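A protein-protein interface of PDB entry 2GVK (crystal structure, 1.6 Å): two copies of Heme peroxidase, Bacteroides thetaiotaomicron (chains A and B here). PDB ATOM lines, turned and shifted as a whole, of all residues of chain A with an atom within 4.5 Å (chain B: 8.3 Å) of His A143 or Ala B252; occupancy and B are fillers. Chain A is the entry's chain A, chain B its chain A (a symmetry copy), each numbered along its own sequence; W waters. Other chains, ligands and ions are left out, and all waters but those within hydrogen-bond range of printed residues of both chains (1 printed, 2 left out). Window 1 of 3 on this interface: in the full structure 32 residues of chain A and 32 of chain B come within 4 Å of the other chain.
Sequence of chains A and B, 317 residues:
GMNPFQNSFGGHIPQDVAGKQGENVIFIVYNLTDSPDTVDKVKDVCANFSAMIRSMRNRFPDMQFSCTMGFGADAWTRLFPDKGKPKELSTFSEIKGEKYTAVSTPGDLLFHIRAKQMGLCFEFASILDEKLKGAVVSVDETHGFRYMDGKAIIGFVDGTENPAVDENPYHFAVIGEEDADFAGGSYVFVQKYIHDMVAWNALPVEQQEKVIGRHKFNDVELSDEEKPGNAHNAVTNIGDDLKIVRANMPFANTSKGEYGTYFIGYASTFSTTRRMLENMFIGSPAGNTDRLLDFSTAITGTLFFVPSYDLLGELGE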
ATOM      1  N   VAL A  25       8.502 -18.786   7.856  1.00  0.00           N
ATOM      2  CA  VAL A  25       8.174 -19.969   8.654  1.00  0.00           C
ATOM      3  C   VAL A  25       7.836 -21.166   7.794  1.00  0.00           C
ATOM      4  O   VAL A  25       7.253 -21.039   6.753  1.00  0.00           O
ATOM      5  CB  VAL A  25       6.973 -19.678   9.650  1.00  0.00           C
ATOM      6  CG1 VAL A  25       5.701 -19.389   8.898  1.00  0.00           C
ATOM      7  CG2 VAL A  25       6.768 -20.845  10.619  1.00  0.00           C
ATOM      8  N   ILE A  26       8.266 -22.337   8.257  1.00  0.00           N
ATOM      9  CA  ILE A  26       7.882 -23.598   7.667  1.00  0.00           C
ATOM     10  C   ILE A  26       7.235 -24.432   8.741  1.00  0.00           C
ATOM     11  O   ILE A  26       7.775 -24.562   9.853  1.00  0.00           O
ATOM     12  CB  ILE A  26       9.087 -24.385   7.106  1.00  0.00           C
ATOM     13  CG1 ILE A  26       9.758 -23.616   5.979  1.00  0.00           C
ATOM     14  CG2 ILE A  26       8.618 -25.738   6.605  1.00  0.00           C
ATOM     15  CD1 ILE A  26      10.961 -24.306   5.398  1.00  0.00           C
ATOM     16  N   MET A 118      14.168 -17.218   4.608  1.00  0.00           N
ATOM     17  CA  MET A 118      13.568 -18.514   4.297  1.00  0.00           C
ATOM     18  C   MET A 118      14.611 -19.569   3.939  1.00  0.00           C
ATOM     19  O   MET A 118      14.417 -20.750   4.217  1.00  0.00           O
ATOM     20  CB  MET A 118      12.546 -18.381   3.172  1.00  0.00           C
ATOM     21  CG  MET A 118      11.906 -19.678   2.777  1.00  0.00           C
ATOM     22  SD  MET A 118      10.961 -20.530   4.277  1.00  0.00           S
ATOM     23  CE  MET A 118       9.133 -19.884   3.912  1.00  0.00           C
ATOM     24  N   PHE A 122      14.814 -23.522   5.027  1.00  0.00           N
ATOM     25  CA  PHE A 122      15.002 -24.584   4.039  1.00  0.00           C
ATOM     26  C   PHE A 122      16.192 -25.449   4.391  1.00  0.00           C
ATOM     27  O   PHE A 122      16.116 -26.653   4.332  1.00  0.00           O
ATOM     28  CB  PHE A 122      15.193 -24.009   2.614  1.00  0.00           C
ATOM     29  CG  PHE A 122      15.810 -24.976   1.664  1.00  0.00           C
ATOM     30  CD1 PHE A 122      15.059 -25.991   1.111  1.00  0.00           C
ATOM     31  CD2 PHE A 122      17.180 -24.938   1.390  1.00  0.00           C
ATOM     32  CE1 PHE A 122      15.641 -26.924   0.291  1.00  0.00           C
ATOM     33  CE2 PHE A 122      17.762 -25.861   0.537  1.00  0.00           C
ATOM     34  CZ  PHE A 122      16.994 -26.871   0.012  1.00  0.00           C
ATOM     35  N   GLU A 141       2.880 -29.661   4.557  1.00  0.00           N
ATOM     36  CA  GLU A 141       3.914 -28.620   4.644  1.00  0.00           C
ATOM     37  C   GLU A 141       3.313 -27.311   4.221  1.00  0.00           C
ATOM     38  O   GLU A 141       2.699 -27.214   3.154  1.00  0.00           O
ATOM     39  CB  GLU A 141       5.119 -28.943   3.765  1.00  0.00           C
ATOM     40  CG  GLU A 141       6.222 -27.894   3.846  1.00  0.00           C
ATOM     41  CD  GLU A 141       7.545 -28.340   3.187  1.00  0.00           C
ATOM     42  OE1 GLU A 141       7.764 -29.564   3.019  1.00  0.00           O
ATOM     43  OE2 GLU A 141       8.346 -27.447   2.810  1.00  0.00           O
ATOM     44  N   THR A 142       3.403 -26.331   5.097  1.00  0.00           N
ATOM     45  CA  THR A 142       2.910 -25.005   4.814  1.00  0.00           C
ATOM     46  C   THR A 142       4.009 -23.990   5.063  1.00  0.00           C
ATOM     47  O   THR A 142       4.734 -24.057   6.080  1.00  0.00           O
ATOM     48  CB  THR A 142       1.677 -24.663   5.688  1.00  0.00           C
ATOM     49  OG1 THR A 142       0.623 -25.610   5.428  1.00  0.00           O
ATOM     50  CG2 THR A 142       1.169 -23.268   5.385  1.00  0.00           C
ATOM     51  N   HIS A 143       4.161 -23.067   4.120  1.00  0.00           N
ATOM     52  CA  HIS A 143       5.110 -21.987   4.259  1.00  0.00           C
ATOM     53  C   HIS A 143       4.381 -20.717   4.591  1.00  0.00           C
ATOM     54  O   HIS A 143       3.433 -20.350   3.912  1.00  0.00           O
ATOM     55  CB  HIS A 143       5.890 -21.798   2.978  1.00  0.00           C
ATOM     56  CG  HIS A 143       6.646 -23.003   2.553  1.00  0.00           C
ATOM     57  ND1 HIS A 143       7.131 -23.163   1.279  1.00  0.00           N
ATOM     58  CD2 HIS A 143       6.944 -24.143   3.215  1.00  0.00           C
ATOM     59  CE1 HIS A 143       7.735 -24.338   1.187  1.00  0.00           C
ATOM     60  NE2 HIS A 143       7.627 -24.952   2.347  1.00  0.00           N
ATOM     61  N   GLY A 144       4.846 -20.026   5.613  1.00  0.00           N
ATOM     62  CA  GLY A 144       4.220 -18.778   6.051  1.00  0.00           C
ATOM     63  C   GLY A 144       5.172 -17.606   6.007  1.00  0.00           C
ATOM     64  O   GLY A 144       6.380 -17.765   5.781  1.00  0.00           O
ATOM     65  N   PRO A 250       0.194 -16.085   8.287  1.00  0.00           N
ATOM     66  CA  PRO A 250      -0.363 -16.073   6.954  1.00  0.00           C
ATOM     67  C   PRO A 250       0.279 -17.116   6.024  1.00  0.00           C
ATOM     68  O   PRO A 250       1.475 -17.346   6.083  1.00  0.00           O
ATOM     69  CB  PRO A 250      -0.024 -14.659   6.444  1.00  0.00           C
ATOM     70  CG  PRO A 250       0.189 -13.859   7.624  1.00  0.00           C
ATOM     71  CD  PRO A 250       0.694 -14.757   8.686  1.00  0.00           C
ATOM     72  N   PHE A 251      -0.536 -17.726   5.175  1.00  0.00           N
ATOM     73  CA  PHE A 251      -0.037 -18.479   4.022  1.00  0.00           C
ATOM     74  C   PHE A 251      -1.008 -18.283   2.865  1.00  0.00           C
ATOM     75  O   PHE A 251      -2.196 -17.972   3.080  1.00  0.00           O
ATOM     76  CB  PHE A 251       0.158 -19.956   4.340  1.00  0.00           C
ATOM     77  CG  PHE A 251      -1.114 -20.706   4.602  1.00  0.00           C
ATOM     78  CD1 PHE A 251      -1.613 -20.827   5.886  1.00  0.00           C
ATOM     79  CD2 PHE A 251      -1.749 -21.375   3.588  1.00  0.00           C
ATOM     80  CE1 PHE A 251      -2.771 -21.596   6.139  1.00  0.00           C
ATOM     81  CE2 PHE A 251      -2.894 -22.113   3.824  1.00  0.00           C
ATOM     82  CZ  PHE A 251      -3.388 -22.234   5.135  1.00  0.00           C
ATOM     83  N   MET B 118       8.772 -11.507   1.928  1.00  0.00           N
ATOM     84  CA  MET B 118       7.747 -12.240   1.189  1.00  0.00           C
ATOM     85  C   MET B 118       6.364 -11.609   1.326  1.00  0.00           C
ATOM     86  O   MET B 118       5.558 -11.677   0.401  1.00  0.00           O
ATOM     87  CB  MET B 118       7.705 -13.702   1.625  1.00  0.00           C
ATOM     88  CG  MET B 118       6.656 -14.513   0.927  1.00  0.00           C
ATOM     89  SD  MET B 118       6.903 -14.533  -1.024  1.00  0.00           S
ATOM     90  CE  MET B 118       7.886 -16.233  -1.206  1.00  0.00           C
ATOM     91  N   THR B 142       4.873 -20.700  -8.045  1.00  0.00           N
ATOM     92  CA  THR B 142       6.024 -21.204  -7.337  1.00  0.00           C
ATOM     93  C   THR B 142       6.623 -20.100  -6.488  1.00  0.00           C
ATOM     94  O   THR B 142       6.771 -18.943  -6.940  1.00  0.00           O
ATOM     95  CB  THR B 142       7.095 -21.748  -8.316  1.00  0.00           C
ATOM     96  OG1 THR B 142       6.534 -22.818  -9.100  1.00  0.00           O
ATOM     97  CG2 THR B 142       8.300 -22.273  -7.562  1.00  0.00           C
ATOM     98  N   HIS B 143       6.938 -20.441  -5.242  1.00  0.00           N
ATOM     99  CA  HIS B 143       7.593 -19.518  -4.344  1.00  0.00           C
ATOM    100  C   HIS B 143       9.041 -19.890  -4.211  1.00  0.00           C
ATOM    101  O   HIS B 143       9.365 -21.036  -3.936  1.00  0.00           O
ATOM    102  CB  HIS B 143       6.938 -19.550  -2.981  1.00  0.00           C
ATOM    103  CG  HIS B 143       5.495 -19.203  -3.002  1.00  0.00           C
ATOM    104  ND1 HIS B 143       4.648 -19.495  -1.962  1.00  0.00           N
ATOM    105  CD2 HIS B 143       4.729 -18.648  -3.967  1.00  0.00           C
ATOM    106  CE1 HIS B 143       3.424 -19.094  -2.270  1.00  0.00           C
ATOM    107  NE2 HIS B 143       3.449 -18.584  -3.484  1.00  0.00           N
ATOM    108  N   GLY B 144       9.912 -18.913  -4.369  1.00  0.00           N
ATOM    109  CA  GLY B 144      11.355 -19.142  -4.279  1.00  0.00           C
ATOM    110  C   GLY B 144      12.006 -18.312  -3.197  1.00  0.00           C
ATOM    111  O   GLY B 144      11.378 -17.429  -2.596  1.00  0.00           O
ATOM    112  N   PHE B 145      13.265 -18.618  -2.916  1.00  0.00           N
ATOM    113  CA  PHE B 145      14.009 -17.925  -1.872  1.00  0.00           C
ATOM    114  C   PHE B 145      15.456 -17.878  -2.245  1.00  0.00           C
ATOM    115  O   PHE B 145      15.958 -18.786  -2.908  1.00  0.00           O
ATOM    116  CB  PHE B 145      13.852 -18.656  -0.526  1.00  0.00           C
ATOM    117  CG  PHE B 145      14.202 -20.115  -0.585  1.00  0.00           C
ATOM    118  CD1 PHE B 145      13.255 -21.054  -0.929  1.00  0.00           C
ATOM    119  CD2 PHE B 145      15.504 -20.542  -0.340  1.00  0.00           C
ATOM    120  CE1 PHE B 145      13.599 -22.395  -1.024  1.00  0.00           C
ATOM    121  CE2 PHE B 145      15.834 -21.850  -0.425  1.00  0.00           C
ATOM    122  CZ  PHE B 145      14.890 -22.785  -0.766  1.00  0.00           C
ATOM    123  N   ILE B 153      20.029 -24.381  -5.538  1.00  0.00           N
ATOM    124  CA  ILE B 153      19.630 -25.369  -4.557  1.00  0.00           C
ATOM    125  C   ILE B 153      20.595 -26.593  -4.558  1.00  0.00           C
ATOM    126  O   ILE B 153      20.661 -27.345  -3.580  1.00  0.00           O
ATOM    127  CB  ILE B 153      18.162 -25.788  -4.801  1.00  0.00           C
ATOM    128  CG1 ILE B 153      17.524 -26.352  -3.514  1.00  0.00           C
ATOM    129  CG2 ILE B 153      18.063 -26.757  -5.958  1.00  0.00           C
ATOM    130  CD1 ILE B 153      16.024 -26.427  -3.589  1.00  0.00           C
ATOM    131  N   ILE B 194      13.086 -30.014 -11.784  1.00  0.00           N
ATOM    132  CA  ILE B 194      13.060 -30.862 -10.576  1.00  0.00           C
ATOM    133  C   ILE B 194      14.359 -31.642 -10.506  1.00  0.00           C
ATOM    134  O   ILE B 194      14.765 -32.265 -11.485  1.00  0.00           O
ATOM    135  CB  ILE B 194      11.870 -31.826 -10.602  1.00  0.00           C
ATOM    136  CG1 ILE B 194      10.546 -31.035 -10.747  1.00  0.00           C
ATOM    137  CG2 ILE B 194      11.846 -32.705  -9.346  1.00  0.00           C
ATOM    138  CD1 ILE B 194      10.282 -30.052  -9.628  1.00  0.00           C
ATOM    139  N   MET B 197      18.069 -34.991  -6.127  1.00  0.00           N
ATOM    140  CA  MET B 197      19.016 -34.582  -5.067  1.00  0.00           C
ATOM    141  C   MET B 197      19.752 -35.741  -4.451  1.00  0.00           C
ATOM    142  O   MET B 197      20.877 -35.598  -4.031  1.00  0.00           O
ATOM    143  CB  MET B 197      18.296 -33.797  -3.977  1.00  0.00           C
ATOM    144  CG  MET B 197      17.773 -32.519  -4.440  1.00  0.00           C
ATOM    145  SD  MET B 197      19.167 -31.346  -5.174  1.00  0.00           S
ATOM    146  CE  MET B 197      19.815 -30.580  -3.513  1.00  0.00           C
ATOM    147  N   MET B 249      16.282 -19.771  -9.326  1.00  0.00           N
ATOM    148  CA  MET B 249      15.792 -19.570  -7.967  1.00  0.00           C
ATOM    149  C   MET B 249      15.379 -20.894  -7.357  1.00  0.00           C
ATOM    150  O   MET B 249      14.596 -21.634  -7.939  1.00  0.00           O
ATOM    151  CB  MET B 249      14.590 -18.627  -7.961  1.00  0.00           C
ATOM    152  CG  MET B 249      14.908 -17.214  -8.401  1.00  0.00           C
ATOM    153  SD  MET B 249      16.510 -16.530  -7.524  1.00  0.00           S
ATOM    154  CE  MET B 249      15.762 -16.107  -5.838  1.00  0.00           C
ATOM    155  N   PRO B 250      15.906 -21.179  -6.174  1.00  0.00           N
ATOM    156  CA  PRO B 250      15.519 -22.369  -5.452  1.00  0.00           C
ATOM    157  C   PRO B 250      14.029 -22.384  -5.070  1.00  0.00           C
ATOM    158  O   PRO B 250      13.470 -21.359  -4.718  1.00  0.00           O
ATOM    159  CB  PRO B 250      16.373 -22.294  -4.171  1.00  0.00           C
ATOM    160  CG  PRO B 250      17.487 -21.439  -4.493  1.00  0.00           C
ATOM    161  CD  PRO B 250      17.030 -20.481  -5.524  1.00  0.00           C
ATOM    162  N   PHE B 251      13.417 -23.557  -5.145  1.00  0.00           N
ATOM    163  CA  PHE B 251      12.120 -23.800  -4.507  1.00  0.00           C
ATOM    164  C   PHE B 251      12.101 -25.232  -3.992  1.00  0.00           C
ATOM    165  O   PHE B 251      12.845 -26.097  -4.494  1.00  0.00           O
ATOM    166  CB  PHE B 251      10.956 -23.532  -5.453  1.00  0.00           C
ATOM    167  CG  PHE B 251      10.858 -24.493  -6.601  1.00  0.00           C
ATOM    168  CD1 PHE B 251      11.478 -24.220  -7.806  1.00  0.00           C
ATOM    169  CD2 PHE B 251      10.064 -25.606  -6.510  1.00  0.00           C
ATOM    170  CE1 PHE B 251      11.323 -25.091  -8.909  1.00  0.00           C
ATOM    171  CE2 PHE B 251       9.923 -26.473  -7.578  1.00  0.00           C
ATOM    172  CZ  PHE B 251      10.554 -26.183  -8.801  1.00  0.00           C
ATOM    173  N   ALA B 252      11.317 -25.482  -2.951  1.00  0.00           N
ATOM    174  CA  ALA B 252      11.296 -26.817  -2.366  1.00  0.00           C
ATOM    175  C   ALA B 252      10.161 -27.079  -1.458  1.00  0.00           C
ATOM    176  O   ALA B 252       9.676 -26.171  -0.760  1.00  0.00           O
ATOM    177  CB  ALA B 252      12.603 -27.063  -1.589  1.00  0.00           C
ATOM    178  N   ASN B 253       9.748 -28.345  -1.448  1.00  0.00           N
ATOM    179  CA  ASN B 253       8.895 -28.911  -0.392  1.00  0.00           C
ATOM    180  C   ASN B 253       9.651 -30.102   0.178  1.00  0.00           C
ATOM    181  O   ASN B 253       9.499 -31.218  -0.299  1.00  0.00           O
ATOM    182  CB  ASN B 253       7.529 -29.351  -0.953  1.00  0.00           C
ATOM    183  CG  ASN B 253       6.601 -29.914   0.122  1.00  0.00           C
ATOM    184  OD1 ASN B 253       7.057 -30.521   1.107  1.00  0.00           O
ATOM    185  ND2 ASN B 253       5.276 -29.735  -0.072  1.00  0.00           N
ATOM    186  N   THR B 254      10.557 -29.842   1.115  1.00  0.00           N
ATOM    187  CA  THR B 254      11.474 -30.872   1.603  1.00  0.00           C
ATOM    188  C   THR B 254      10.763 -32.053   2.260  1.00  0.00           C
ATOM    189  O   THR B 254      11.257 -33.149   2.239  1.00  0.00           O
ATOM    190  CB  THR B 254      12.497 -30.299   2.579  1.00  0.00           C
ATOM    191  OG1 THR B 254      11.826 -29.704   3.683  1.00  0.00           O
ATOM    192  CG2 THR B 254      13.353 -29.251   1.890  1.00  0.00           C
ATOM    193  N   SER B 255       9.584 -31.808   2.828  1.00  0.00           N
ATOM    194  CA  SER B 255       8.846 -32.872   3.508  1.00  0.00           C
ATOM    195  C   SER B 255       8.459 -33.971   2.515  1.00  0.00           C
ATOM    196  O   SER B 255       8.337 -35.134   2.888  1.00  0.00           O
ATOM    197  CB  SER B 255       7.597 -32.308   4.224  1.00  0.00           C
ATOM    198  OG  SER B 255       6.550 -32.018   3.320  1.00  0.00           O
ATOM    199  N   LYS B 256       8.316 -33.583   1.229  1.00  0.00           N
ATOM    200  CA  LYS B 256       8.000 -34.526   0.124  1.00  0.00           C
ATOM    201  C   LYS B 256       9.240 -34.895  -0.675  1.00  0.00           C
ATOM    202  O   LYS B 256       9.148 -35.597  -1.702  1.00  0.00           O
ATOM    203  CB  LYS B 256       6.965 -33.906  -0.811  1.00  0.00           C
ATOM    204  CG  LYS B 256       5.634 -33.672  -0.162  1.00  0.00           C
ATOM    205  CD  LYS B 256       4.648 -32.931  -1.109  1.00  0.00           C
ATOM    206  N   GLY B 257      10.398 -34.442  -0.216  1.00  0.00           N
ATOM    207  CA  GLY B 257      11.647 -34.682  -0.917  1.00  0.00           C
ATOM    208  C   GLY B 257      11.720 -33.979  -2.264  1.00  0.00           C
ATOM    209  O   GLY B 257      12.428 -34.429  -3.158  1.00  0.00           O
ATOM    210  N   GLU B 258      11.010 -32.854  -2.396  1.00  0.00           N
ATOM    211  CA  GLU B 258      10.927 -32.112  -3.673  1.00  0.00           C
ATOM    212  C   GLU B 258      11.864 -30.930  -3.660  1.00  0.00           C
ATOM    213  O   GLU B 258      11.697 -30.010  -2.859  1.00  0.00           O
ATOM    214  CB  GLU B 258       9.491 -31.613  -3.924  1.00  0.00           C
ATOM    215  CG  GLU B 258       9.339 -30.770  -5.216  1.00  0.00           C
ATOM    216  CD  GLU B 258       8.024 -29.955  -5.273  1.00  0.00           C
ATOM    217  OE1 GLU B 258       7.203 -30.062  -4.340  1.00  0.00           O
ATOM    218  OE2 GLU B 258       7.825 -29.221  -6.265  1.00  0.00           O
ATOM    219  N   TYR B 259      12.847 -30.947  -4.566  1.00  0.00           N
ATOM    220  CA  TYR B 259      13.837 -29.882  -4.676  1.00  0.00           C
ATOM    221  C   TYR B 259      13.891 -29.430  -6.112  1.00  0.00           C
ATOM    222  O   TYR B 259      14.024 -30.266  -7.028  1.00  0.00           O
ATOM    223  CB  TYR B 259      15.212 -30.364  -4.266  1.00  0.00           C
ATOM    224  CG  TYR B 259      15.305 -30.827  -2.830  1.00  0.00           C
ATOM    225  CD1 TYR B 259      14.901 -32.099  -2.468  1.00  0.00           C
ATOM    226  CD2 TYR B 259      15.843 -30.015  -1.860  1.00  0.00           C
ATOM    227  CE1 TYR B 259      14.963 -32.519  -1.160  1.00  0.00           C
ATOM    228  CE2 TYR B 259      15.947 -30.448  -0.549  1.00  0.00           C
ATOM    229  CZ  TYR B 259      15.505 -31.700  -0.212  1.00  0.00           C
ATOM    230  OH  TYR B 259      15.579 -32.113   1.115  1.00  0.00           O
ATOM    231  N   GLY B 260      13.800 -28.127  -6.326  1.00  0.00           N
ATOM    232  CA  GLY B 260      13.787 -27.593  -7.685  1.00  0.00           C
ATOM    233  C   GLY B 260      14.487 -26.264  -7.891  1.00  0.00           C
ATOM    234  O   GLY B 260      14.892 -25.591  -6.947  1.00  0.00           O
ATOM    235  N   THR B 261      14.688 -25.944  -9.168  1.00  0.00           N
ATOM    236  CA  THR B 261      15.216 -24.673  -9.604  1.00  0.00           C
ATOM    237  C   THR B 261      14.209 -24.068 -10.569  1.00  0.00           C
ATOM    238  O   THR B 261      13.761 -24.732 -11.517  1.00  0.00           O
ATOM    239  CB  THR B 261      16.558 -24.853 -10.346  1.00  0.00           C
ATOM    240  OG1 THR B 261      17.571 -25.236  -9.426  1.00  0.00           O
ATOM    241  CG2 THR B 261      16.969 -23.575 -11.032  1.00  0.00           C
ATOM    242  N   TYR B 262      13.818 -22.826 -10.318  1.00  0.00           N
ATOM    243  CA  TYR B 262      12.983 -22.104 -11.242  1.00  0.00           C
ATOM    244  C   TYR B 262      13.879 -21.209 -12.080  1.00  0.00           C
ATOM    245  O   TYR B 262      14.425 -20.221 -11.590  1.00  0.00           O
ATOM    246  CB  TYR B 262      11.914 -21.275 -10.486  1.00  0.00           C
ATOM    247  CG  TYR B 262      10.700 -20.912 -11.333  1.00  0.00           C
ATOM    248  CD1 TYR B 262      10.793 -19.939 -12.324  1.00  0.00           C
ATOM    249  CD2 TYR B 262       9.474 -21.564 -11.167  1.00  0.00           C
ATOM    250  CE1 TYR B 262       9.730 -19.632 -13.119  1.00  0.00           C
ATOM    251  CE2 TYR B 262       8.386 -21.247 -11.967  1.00  0.00           C
ATOM    252  CZ  TYR B 262       8.539 -20.284 -12.960  1.00  0.00           C
ATOM    253  OH  TYR B 262       7.469 -19.931 -13.770  1.00  0.00           O
HETATM  254  O   HOH W   1      10.798 -27.351   3.041  1.00  0.00           O
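The side-chain carboxylate of Glu A141 lies within hydrogen-bond range of the backbone NH of Thr B254. OG of Ser B255 is in hydrogen-bond range of OE1 of Glu A141, at 2.8 Å. OE1 of Glu A141 sits close to OD1 of Asn B253, at 2.3 Å.
N of Phe B145 sits at hydrogen-bond distance from O of Pro B250. The backbone NH of Lys B256 sits at hydrogen-bond distance from the side-chain amide oxygen of Asn B253 (3.3 Å). The side-chain amide oxygen (OD1) of Asn B253 is in hydrogen-bond range of the side-chain hydroxyl (OG) of Ser B255, 2.7 Å away. NE2 of His A143 is in hydrogen-bond range of OE2 of Glu A141. The backbone carbonyl oxygen (O) of Glu B258 lies within hydrogen-bond range of the backbone NH (N) of Asn B253 (2.9 Å).
Met A118 touches Phe B145 (CB to CB, 3.9 Å). CZ of Phe B145 touches CG of Phe A122, 3.4 Å away. CZ of Phe A122 touches CG1 of Ile B153, at 3.6 Å. CE1 of Phe A122 touches CB of Ala B252, at 3.6 Å. Phe A122 touches Thr B254 (CE1 to CG2, 3.6 Å). CE1 of Phe A122 touches CE2 of Tyr B259, 3.6 Å away. O of Ala B252 touches CE1 of His A143 (3.3 Å).
Of the printed residues of chain B, His A143 touches Ala B252 (3.3 Å). Of the printed residues of chain A, Asn B253 touches Glu A141. Printed residues of chain A within 4 Å of Phe B145: Met A118 (3.9 Å) and Phe A122 (3.4 Å). Of the printed residues of chain B, Met A118 touches Phe B145 (3.9 Å). Printed residues of chain A within 4 Å of Thr B254: Phe A122 (3.6 Å) and Glu A141 (3.4 Å). Printed residues of chain B within 4 Å of Glu A141: Asn B253 (2.3 Å), Thr B254 (3.4 Å) and Ser B255 (2.8 Å). Pro B250 touches none of the printed residues of chain A. The nearest printed residue of chain B that does not touch His A143 is Asn B253 (5.0 Å). The nearest printed residue of chain A that does not touch Ala B252 is Glu A141 (4.02 Å). The nearest printed residue of chain B that does not touch Glu A141 is Ala B252 (4.02 Å).
Printed residues of chain B that touch a printed residue of chain A: Phe B145, Ile B153, Ala B252, Asn B253, Thr B254, Ser B255 and Tyr B259. Hydrophobic or aromatic side chains of chain A that line the printed part of chain B: Met A118, Phe A122 and His A143. Along chain A the printed residues that touch a printed residue of chain B span positions 118 to 143. Among the printed residues, no Asp or Glu carboxylate lies within 4 Å of a Lys or Arg side-chain nitrogen of the other chain.
Positions printed for both chains: 118, 142, 143, 144, 250 and 251. Of the 10 pairs that touch across the chains among the printed residues, none has its exchanged pair printed and touching as well.
Water W1 lies within hydrogen-bond range of OE2 of Glu A141 and OG1 of Thr B254.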
